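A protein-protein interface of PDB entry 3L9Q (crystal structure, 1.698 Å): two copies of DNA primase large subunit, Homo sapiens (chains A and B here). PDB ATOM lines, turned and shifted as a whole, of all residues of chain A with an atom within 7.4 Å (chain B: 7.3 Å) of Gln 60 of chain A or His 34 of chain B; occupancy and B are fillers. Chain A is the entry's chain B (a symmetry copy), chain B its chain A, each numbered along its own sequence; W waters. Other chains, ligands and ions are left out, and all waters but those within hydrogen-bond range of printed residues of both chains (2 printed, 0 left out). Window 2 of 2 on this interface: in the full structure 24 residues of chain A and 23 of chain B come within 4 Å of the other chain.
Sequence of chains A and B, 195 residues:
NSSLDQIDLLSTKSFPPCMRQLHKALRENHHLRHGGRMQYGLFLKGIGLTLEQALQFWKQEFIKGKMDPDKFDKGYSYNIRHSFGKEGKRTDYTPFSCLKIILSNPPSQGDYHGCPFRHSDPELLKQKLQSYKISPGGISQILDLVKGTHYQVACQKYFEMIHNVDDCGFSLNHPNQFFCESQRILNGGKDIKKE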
ATOM      1  N   GLN A  56      23.456  -0.753 -25.462  1.00  0.00           N
ATOM      2  CA  GLN A  56      22.219  -1.515 -25.582  1.00  0.00           C
ATOM      3  C   GLN A  56      21.239  -1.128 -24.476  1.00  0.00           C
ATOM      4  O   GLN A  56      21.462  -1.440 -23.302  1.00  0.00           O
ATOM      5  CB  GLN A  56      22.533  -3.008 -25.518  1.00  0.00           C
ATOM      6  CG  GLN A  56      23.488  -3.468 -26.616  1.00  0.00           C
ATOM      7  CD  GLN A  56      23.938  -4.902 -26.437  1.00  0.00           C
ATOM      8  OE1 GLN A  56      24.441  -5.278 -25.380  1.00  0.00           O
ATOM      9  NE2 GLN A  56      23.765  -5.711 -27.474  1.00  0.00           N
ATOM     10  N   PHE A  57      20.151  -0.452 -24.844  1.00  0.00           N
ATOM     11  CA  PHE A  57      19.267   0.131 -23.835  1.00  0.00           C
ATOM     12  C   PHE A  57      18.646  -0.905 -22.908  1.00  0.00           C
ATOM     13  O   PHE A  57      18.301  -0.588 -21.765  1.00  0.00           O
ATOM     14  CB  PHE A  57      18.185   1.032 -24.461  1.00  0.00           C
ATOM     15  CG  PHE A  57      17.092   0.286 -25.197  1.00  0.00           C
ATOM     16  CD1 PHE A  57      16.064  -0.331 -24.507  1.00  0.00           C
ATOM     17  CD2 PHE A  57      17.071   0.251 -26.584  1.00  0.00           C
ATOM     18  CE1 PHE A  57      15.042  -1.005 -25.178  1.00  0.00           C
ATOM     19  CE2 PHE A  57      16.057  -0.415 -27.272  1.00  0.00           C
ATOM     20  CZ  PHE A  57      15.038  -1.044 -26.566  1.00  0.00           C
ATOM     21  N   TRP A  58      18.514  -2.135 -23.395  1.00  0.00           N
ATOM     22  CA  TRP A  58      17.818  -3.179 -22.643  1.00  0.00           C
ATOM     23  C   TRP A  58      18.728  -3.892 -21.648  1.00  0.00           C
ATOM     24  O   TRP A  58      18.277  -4.755 -20.894  1.00  0.00           O
ATOM     25  CB  TRP A  58      17.193  -4.199 -23.598  1.00  0.00           C
ATOM     26  CG  TRP A  58      18.192  -4.849 -24.509  1.00  0.00           C
ATOM     27  CD1 TRP A  58      18.812  -6.055 -24.321  1.00  0.00           C
ATOM     28  CD2 TRP A  58      18.680  -4.335 -25.753  1.00  0.00           C
ATOM     29  NE1 TRP A  58      19.659  -6.318 -25.371  1.00  0.00           N
ATOM     30  CE2 TRP A  58      19.599  -5.278 -26.262  1.00  0.00           C
ATOM     31  CE3 TRP A  58      18.439  -3.166 -26.482  1.00  0.00           C
ATOM     32  CZ2 TRP A  58      20.270  -5.090 -27.469  1.00  0.00           C
ATOM     33  CZ3 TRP A  58      19.113  -2.976 -27.681  1.00  0.00           C
ATOM     34  CH2 TRP A  58      20.017  -3.934 -28.162  1.00  0.00           C
ATOM     35  N   LYS A  59      20.007  -3.533 -21.648  1.00  0.00           N
ATOM     36  CA  LYS A  59      20.955  -4.081 -20.680  1.00  0.00           C
ATOM     37  C   LYS A  59      21.023  -3.213 -19.430  1.00  0.00           C
ATOM     38  O   LYS A  59      21.164  -1.994 -19.517  1.00  0.00           O
ATOM     39  CB  LYS A  59      22.352  -4.204 -21.290  1.00  0.00           C
ATOM     40  CG  LYS A  59      22.433  -5.159 -22.461  1.00  0.00           C
ATOM     41  CD  LYS A  59      22.089  -6.578 -22.047  1.00  0.00           C
ATOM     42  CE  LYS A  59      22.232  -7.533 -23.222  1.00  0.00           C
ATOM     43  NZ  LYS A  59      23.558  -7.373 -23.886  1.00  0.00           N
ATOM     44  N   GLN A  60      20.929  -3.853 -18.269  1.00  0.00           N
ATOM     45  CA  GLN A  60      21.004  -3.156 -16.995  1.00  0.00           C
ATOM     46  C   GLN A  60      22.456  -2.765 -16.723  1.00  0.00           C
ATOM     47  O   GLN A  60      23.372  -3.529 -17.024  1.00  0.00           O
ATOM     48  CB  GLN A  60      20.460  -4.060 -15.879  1.00  0.00           C
ATOM     49  CG  GLN A  60      19.823  -3.322 -14.720  1.00  0.00           C
ATOM     50  CD  GLN A  60      18.820  -4.177 -13.963  1.00  0.00           C
ATOM     51  OE1 GLN A  60      18.098  -3.685 -13.097  1.00  0.00           O
ATOM     52  NE2 GLN A  60      18.766  -5.465 -14.294  1.00  0.00           N
ATOM     53  N   GLU A  61      22.672  -1.568 -16.186  1.00  0.00           N
ATOM     54  CA  GLU A  61      24.018  -1.159 -15.792  1.00  0.00           C
ATOM     55  C   GLU A  61      24.297  -1.555 -14.344  1.00  0.00           C
ATOM     56  O   GLU A  61      25.439  -1.831 -13.977  1.00  0.00           O
ATOM     57  CB  GLU A  61      24.225   0.346 -15.973  1.00  0.00           C
ATOM     58  CG  GLU A  61      25.661   0.795 -15.675  1.00  0.00           C
ATOM     59  CD  GLU A  61      25.852   2.304 -15.733  1.00  0.00           C
ATOM     60  OE1 GLU A  61      24.854   3.035 -15.906  1.00  0.00           O
ATOM     61  OE2 GLU A  61      27.011   2.761 -15.600  1.00  0.00           O
ATOM     62  N   PHE A  62      23.247  -1.583 -13.528  1.00  0.00           N
ATOM     63  CA  PHE A  62      23.377  -1.940 -12.120  1.00  0.00           C
ATOM     64  C   PHE A  62      22.339  -2.978 -11.714  1.00  0.00           C
ATOM     65  O   PHE A  62      21.162  -2.660 -11.556  1.00  0.00           O
ATOM     66  CB  PHE A  62      23.253  -0.698 -11.232  1.00  0.00           C
ATOM     67  CG  PHE A  62      24.294   0.353 -11.507  1.00  0.00           C
ATOM     68  CD1 PHE A  62      23.972   1.497 -12.220  1.00  0.00           C
ATOM     69  CD2 PHE A  62      25.594   0.193 -11.056  1.00  0.00           C
ATOM     70  CE1 PHE A  62      24.927   2.466 -12.476  1.00  0.00           C
ATOM     71  CE2 PHE A  62      26.557   1.156 -11.308  1.00  0.00           C
ATOM     72  CZ  PHE A  62      26.223   2.295 -12.022  1.00  0.00           C
ATOM     73  N   HIS B  31      18.583  10.634 -19.989  1.00  0.00           N
ATOM     74  CA  HIS B  31      18.759   9.229 -19.628  1.00  0.00           C
ATOM     75  C   HIS B  31      17.518   8.737 -18.904  1.00  0.00           C
ATOM     76  O   HIS B  31      16.735   9.537 -18.392  1.00  0.00           O
ATOM     77  CB  HIS B  31      19.995   9.041 -18.738  1.00  0.00           C
ATOM     78  CG  HIS B  31      20.401   7.608 -18.559  1.00  0.00           C
ATOM     79  ND1 HIS B  31      20.710   7.068 -17.327  1.00  0.00           N
ATOM     80  CD2 HIS B  31      20.550   6.604 -19.457  1.00  0.00           C
ATOM     81  CE1 HIS B  31      21.032   5.794 -17.473  1.00  0.00           C
ATOM     82  NE2 HIS B  31      20.945   5.487 -18.757  1.00  0.00           N
ATOM     83  N   LEU B  32      17.334   7.421 -18.900  1.00  0.00           N
ATOM     84  CA  LEU B  32      16.317   6.773 -18.093  1.00  0.00           C
ATOM     85  C   LEU B  32      16.989   5.569 -17.472  1.00  0.00           C
ATOM     86  O   LEU B  32      17.856   4.963 -18.098  1.00  0.00           O
ATOM     87  CB  LEU B  32      15.165   6.288 -18.971  1.00  0.00           C
ATOM     88  CG  LEU B  32      14.202   7.321 -19.554  1.00  0.00           C
ATOM     89  CD1 LEU B  32      13.321   6.664 -20.614  1.00  0.00           C
ATOM     90  CD2 LEU B  32      13.346   7.954 -18.453  1.00  0.00           C
ATOM     91  N   ARG B  33      16.601   5.223 -16.249  1.00  0.00           N
ATOM     92  CA  ARG B  33      17.018   3.955 -15.664  1.00  0.00           C
ATOM     93  C   ARG B  33      16.382   2.789 -16.420  1.00  0.00           C
ATOM     94  O   ARG B  33      15.531   2.992 -17.283  1.00  0.00           O
ATOM     95  CB  ARG B  33      16.657   3.910 -14.183  1.00  0.00           C
ATOM     96  CG  ARG B  33      17.463   4.885 -13.338  1.00  0.00           C
ATOM     97  CD  ARG B  33      18.953   4.569 -13.414  1.00  0.00           C
ATOM     98  NE  ARG B  33      19.652   4.948 -12.191  1.00  0.00           N
ATOM     99  CZ  ARG B  33      20.074   4.085 -11.269  1.00  0.00           C
ATOM    100  NH1 ARG B  33      19.884   2.783 -11.431  1.00  0.00           N
ATOM    101  NH2 ARG B  33      20.698   4.528 -10.187  1.00  0.00           N
ATOM    102  N   HIS B  34      16.795   1.568 -16.095  1.00  0.00           N
ATOM    103  CA  HIS B  34      16.456   0.391 -16.900  1.00  0.00           C
ATOM    104  C   HIS B  34      14.952   0.159 -17.098  1.00  0.00           C
ATOM    105  O   HIS B  34      14.507  -0.179 -18.198  1.00  0.00           O
ATOM    106  CB  HIS B  34      17.100  -0.855 -16.292  1.00  0.00           C
ATOM    107  CG  HIS B  34      16.925  -2.088 -17.120  1.00  0.00           C
ATOM    108  ND1 HIS B  34      16.087  -3.118 -16.753  1.00  0.00           N
ATOM    109  CD2 HIS B  34      17.484  -2.456 -18.297  1.00  0.00           C
ATOM    110  CE1 HIS B  34      16.145  -4.073 -17.664  1.00  0.00           C
ATOM    111  NE2 HIS B  34      16.986  -3.697 -18.610  1.00  0.00           N
ATOM    112  N   GLY B  35      14.172   0.329 -16.036  1.00  0.00           N
ATOM    113  CA  GLY B  35      12.731   0.138 -16.139  1.00  0.00           C
ATOM    114  C   GLY B  35      12.096   1.044 -17.180  1.00  0.00           C
ATOM    115  O   GLY B  35      11.161   0.647 -17.892  1.00  0.00           O
ATOM    116  N   GLY B  36      12.606   2.266 -17.276  1.00  0.00           N
ATOM    117  CA  GLY B  36      12.108   3.229 -18.245  1.00  0.00           C
ATOM    118  C   GLY B  36      12.634   2.978 -19.645  1.00  0.00           C
ATOM    119  O   GLY B  36      11.903   3.129 -20.623  1.00  0.00           O
ATOM    120  N   ARG B  37      13.913   2.615 -19.755  1.00  0.00           N
ATOM    121  CA  ARG B  37      14.457   2.255 -21.059  1.00  0.00           C
ATOM    122  C   ARG B  37      13.677   1.078 -21.641  1.00  0.00           C
ATOM    123  O   ARG B  37      13.398   1.038 -22.839  1.00  0.00           O
ATOM    124  CB  ARG B  37      15.955   1.933 -20.975  1.00  0.00           C
ATOM    125  CG  ARG B  37      16.802   3.100 -20.488  1.00  0.00           C
ATOM    126  CD  ARG B  37      18.285   2.879 -20.764  1.00  0.00           C
ATOM    127  NE  ARG B  37      18.835   1.644 -20.197  1.00  0.00           N
ATOM    128  CZ  ARG B  37      19.339   1.539 -18.969  1.00  0.00           C
ATOM    129  NH1 ARG B  37      19.330   2.588 -18.156  1.00  0.00           N
ATOM    130  NH2 ARG B  37      19.838   0.380 -18.541  1.00  0.00           N
ATOM    131  N   MET B  38      13.329   0.118 -20.785  1.00  0.00           N
ATOM    132  CA  MET B  38      12.569  -1.048 -21.232  1.00  0.00           C
ATOM    133  C   MET B  38      11.155  -0.669 -21.648  1.00  0.00           C
ATOM    134  O   MET B  38      10.720  -0.970 -22.763  1.00  0.00           O
ATOM    135  CB  MET B  38      12.536  -2.126 -20.142  1.00  0.00           C
ATOM    136  CG  MET B  38      13.883  -2.800 -19.905  1.00  0.00           C
ATOM    137  SD  MET B  38      14.393  -3.811 -21.312  1.00  0.00           S
ATOM    138  CE  MET B  38      13.244  -5.184 -21.173  1.00  0.00           C
ATOM    139  N   GLN B  39      10.433   0.002 -20.757  1.00  0.00           N
ATOM    140  CA  GLN B  39       9.039   0.349 -21.050  1.00  0.00           C
ATOM    141  C   GLN B  39       8.926   1.248 -22.281  1.00  0.00           C
ATOM    142  O   GLN B  39       8.131   0.974 -23.196  1.00  0.00           O
ATOM    143  CB  GLN B  39       8.381   1.003 -19.837  1.00  0.00           C
ATOM    144  CG  GLN B  39       6.947   1.409 -20.080  1.00  0.00           C
ATOM    145  CD  GLN B  39       6.255   1.890 -18.819  1.00  0.00           C
ATOM    146  OE1 GLN B  39       6.487   1.372 -17.726  1.00  0.00           O
ATOM    147  NE2 GLN B  39       5.388   2.881 -18.968  1.00  0.00           N
ATOM    148  N   TYR B  40       9.729   2.309 -22.323  1.00  0.00           N
ATOM    149  CA  TYR B  40       9.657   3.251 -23.437  1.00  0.00           C
ATOM    150  C   TYR B  40      10.325   2.717 -24.707  1.00  0.00           C
ATOM    151  O   TYR B  40       9.766   2.834 -25.798  1.00  0.00           O
ATOM    152  CB  TYR B  40      10.225   4.618 -23.037  1.00  0.00           C
ATOM    153  CG  TYR B  40      10.039   5.685 -24.090  1.00  0.00           C
ATOM    154  CD1 TYR B  40       8.816   5.851 -24.728  1.00  0.00           C
ATOM    155  CD2 TYR B  40      11.081   6.539 -24.440  1.00  0.00           C
ATOM    156  CE1 TYR B  40       8.637   6.827 -25.689  1.00  0.00           C
ATOM    157  CE2 TYR B  40      10.907   7.526 -25.406  1.00  0.00           C
ATOM    158  CZ  TYR B  40       9.679   7.658 -26.026  1.00  0.00           C
ATOM    159  OH  TYR B  40       9.489   8.622 -26.993  1.00  0.00           O
ATOM    160  N   TYR B  93      12.551  -9.100 -26.706  1.00  0.00           N
ATOM    161  CA  TYR B  93      11.655  -8.534 -25.701  1.00  0.00           C
ATOM    162  C   TYR B  93      10.339  -8.046 -26.306  1.00  0.00           C
ATOM    163  O   TYR B  93      10.315  -7.474 -27.396  1.00  0.00           O
ATOM    164  CB  TYR B  93      12.331  -7.391 -24.940  1.00  0.00           C
ATOM    165  CG  TYR B  93      13.405  -7.826 -23.969  1.00  0.00           C
ATOM    166  CD1 TYR B  93      13.076  -8.448 -22.773  1.00  0.00           C
ATOM    167  CD2 TYR B  93      14.749  -7.592 -24.238  1.00  0.00           C
ATOM    168  CE1 TYR B  93      14.059  -8.838 -21.874  1.00  0.00           C
ATOM    169  CE2 TYR B  93      15.734  -7.978 -23.350  1.00  0.00           C
ATOM    170  CZ  TYR B  93      15.385  -8.599 -22.171  1.00  0.00           C
ATOM    171  OH  TYR B  93      16.368  -8.981 -21.284  1.00  0.00           O
ATOM    172  N   PHE B  96       5.360  -3.902 -23.494  1.00  0.00           N
ATOM    173  CA  PHE B  96       4.543  -4.131 -22.305  1.00  0.00           C
ATOM    174  C   PHE B  96       3.066  -3.785 -22.507  1.00  0.00           C
ATOM    175  O   PHE B  96       2.734  -2.741 -23.064  1.00  0.00           O
ATOM    176  CB  PHE B  96       5.059  -3.269 -21.153  1.00  0.00           C
ATOM    177  CG  PHE B  96       6.470  -3.591 -20.698  1.00  0.00           C
ATOM    178  CD1 PHE B  96       7.247  -4.546 -21.340  1.00  0.00           C
ATOM    179  CD2 PHE B  96       7.025  -2.895 -19.634  1.00  0.00           C
ATOM    180  CE1 PHE B  96       8.550  -4.820 -20.900  1.00  0.00           C
ATOM    181  CE2 PHE B  96       8.322  -3.150 -19.197  1.00  0.00           C
ATOM    182  CZ  PHE B  96       9.087  -4.113 -19.833  1.00  0.00           C
ATOM    183  N   GLY B 110      14.066   6.739  -8.363  1.00  0.00           N
ATOM    184  CA  GLY B 110      14.845   7.128  -9.536  1.00  0.00           C
ATOM    185  C   GLY B 110      14.156   6.844 -10.866  1.00  0.00           C
ATOM    186  O   GLY B 110      14.695   7.151 -11.934  1.00  0.00           O
ATOM    187  N   ASP B 111      12.958   6.271 -10.801  1.00  0.00           N
ATOM    188  CA  ASP B 111      12.301   5.709 -11.980  1.00  0.00           C
ATOM    189  C   ASP B 111      11.167   6.590 -12.496  1.00  0.00           C
ATOM    190  O   ASP B 111      10.443   7.185 -11.705  1.00  0.00           O
ATOM    191  CB  ASP B 111      11.706   4.342 -11.638  1.00  0.00           C
ATOM    192  CG  ASP B 111      12.760   3.294 -11.328  1.00  0.00           C
ATOM    193  OD1 ASP B 111      13.866   3.349 -11.912  1.00  0.00           O
ATOM    194  OD2 ASP B 111      12.466   2.390 -10.514  1.00  0.00           O
ATOM    195  N   HIS B 113       9.060   5.188 -14.991  1.00  0.00           N
ATOM    196  CA  HIS B 113       8.180   4.245 -15.672  1.00  0.00           C
ATOM    197  C   HIS B 113       6.897   4.001 -14.876  1.00  0.00           C
ATOM    198  O   HIS B 113       6.617   4.701 -13.897  1.00  0.00           O
ATOM    199  CB  HIS B 113       8.915   2.932 -15.989  1.00  0.00           C
ATOM    200  CG  HIS B 113       9.373   2.177 -14.779  1.00  0.00           C
ATOM    201  ND1 HIS B 113       8.566   1.280 -14.113  1.00  0.00           N
ATOM    202  CD2 HIS B 113      10.559   2.173 -14.125  1.00  0.00           C
ATOM    203  CE1 HIS B 113       9.234   0.755 -13.102  1.00  0.00           C
ATOM    204  NE2 HIS B 113      10.446   1.284 -13.083  1.00  0.00           N
HETATM  205  O   HOH W   1      18.209  -7.306 -20.451  1.00  0.00           O
HETATM  206  O   HOH W   2      22.308   0.318 -20.992  1.00  0.00           O
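The backbone carbonyl oxygen (O) of Phe 57 of chain A sits at hydrogen-bond distance from the guanidinium group (NE) of Arg 37 of chain B. O of Trp 58 of chain A lies within hydrogen-bond range of NE2 of His 34 of chain B (2.8 Å). NH2 of Arg 37 of chain B is in hydrogen-bond range of O of Lys 59 of chain A (2.9 Å).
SD of Met 38 of chain B sits close to NE2 of His 34 of chain B, at 3.7 Å. The side-chain amide oxygen (OE1) of Gln 56 of chain A lies within hydrogen-bond range of the side-chain amino group (NZ) of Lys 59 of chain A, 2.7 Å away. The guanidinium group (NH1) of Arg 37 of chain B sits at hydrogen-bond distance from the backbone carbonyl oxygen (O) of Leu 32 of chain B, at 2.8 Å. NE2 of His 31 of chain B lies within hydrogen-bond range of NH1 of Arg 37 of chain B (3.4 Å).
Among the printed residues, merely in contact across the chains: Trp 58 of chain A with Met 38 of chain B, Trp 58 of chain A with Tyr 93 of chain B, Lys 59 of chain A with His 34 of chain B and Gln 60 of chain A with His 34 of chain B.
Of the printed residues of chain B, Phe 57 of chain A touches Arg 37 (2.8 Å). Printed residues of chain B within 4 Å of Trp 58 of chain A: His 34 (2.8 Å), Met 38 (3.6 Å) and Tyr 93 (3.8 Å). Leu 32 of chain B touches none of the printed residues of chain A. Gly 36 of chain B touches none of the printed residues of chain A. The nearest residue of chain B that does not touch Gln 60 of chain A is Arg 37 of chain B (4.03 Å). The nearest residue of chain A that does not touch His 34 of chain B is Phe 57 of chain A (4.02 Å).
Hydrophobic or aromatic side chains of chain B that line the printed part of chain A: His 34, Met 38 and Tyr 93. Of the 7 printed residues of chain A, 4 touch a printed residue of chain B. Hydrophobic or aromatic side chains of chain A that line the printed part of chain B: Phe 57 and Trp 58. Among the printed residues, no Asp or Glu carboxylate lies within 4 Å of a Lys or Arg side-chain nitrogen of the other chain.
No position is printed for both chains. Of the 7 pairs that touch across the chains among the printed residues, none has its exchanged pair printed and touching as well.
Water W1 bridges O of Trp 58 of chain A and OH of Tyr 93 of chain B. Water W2 lies within hydrogen-bond range of the backbone carbonyl oxygen of Lys 59 of chain A (3.0 Å), the backbone carbonyl oxygen of Gln 56 of chain A (3.0 Å) and the guanidinium group of Arg 37 of chain B (3.5 Å).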
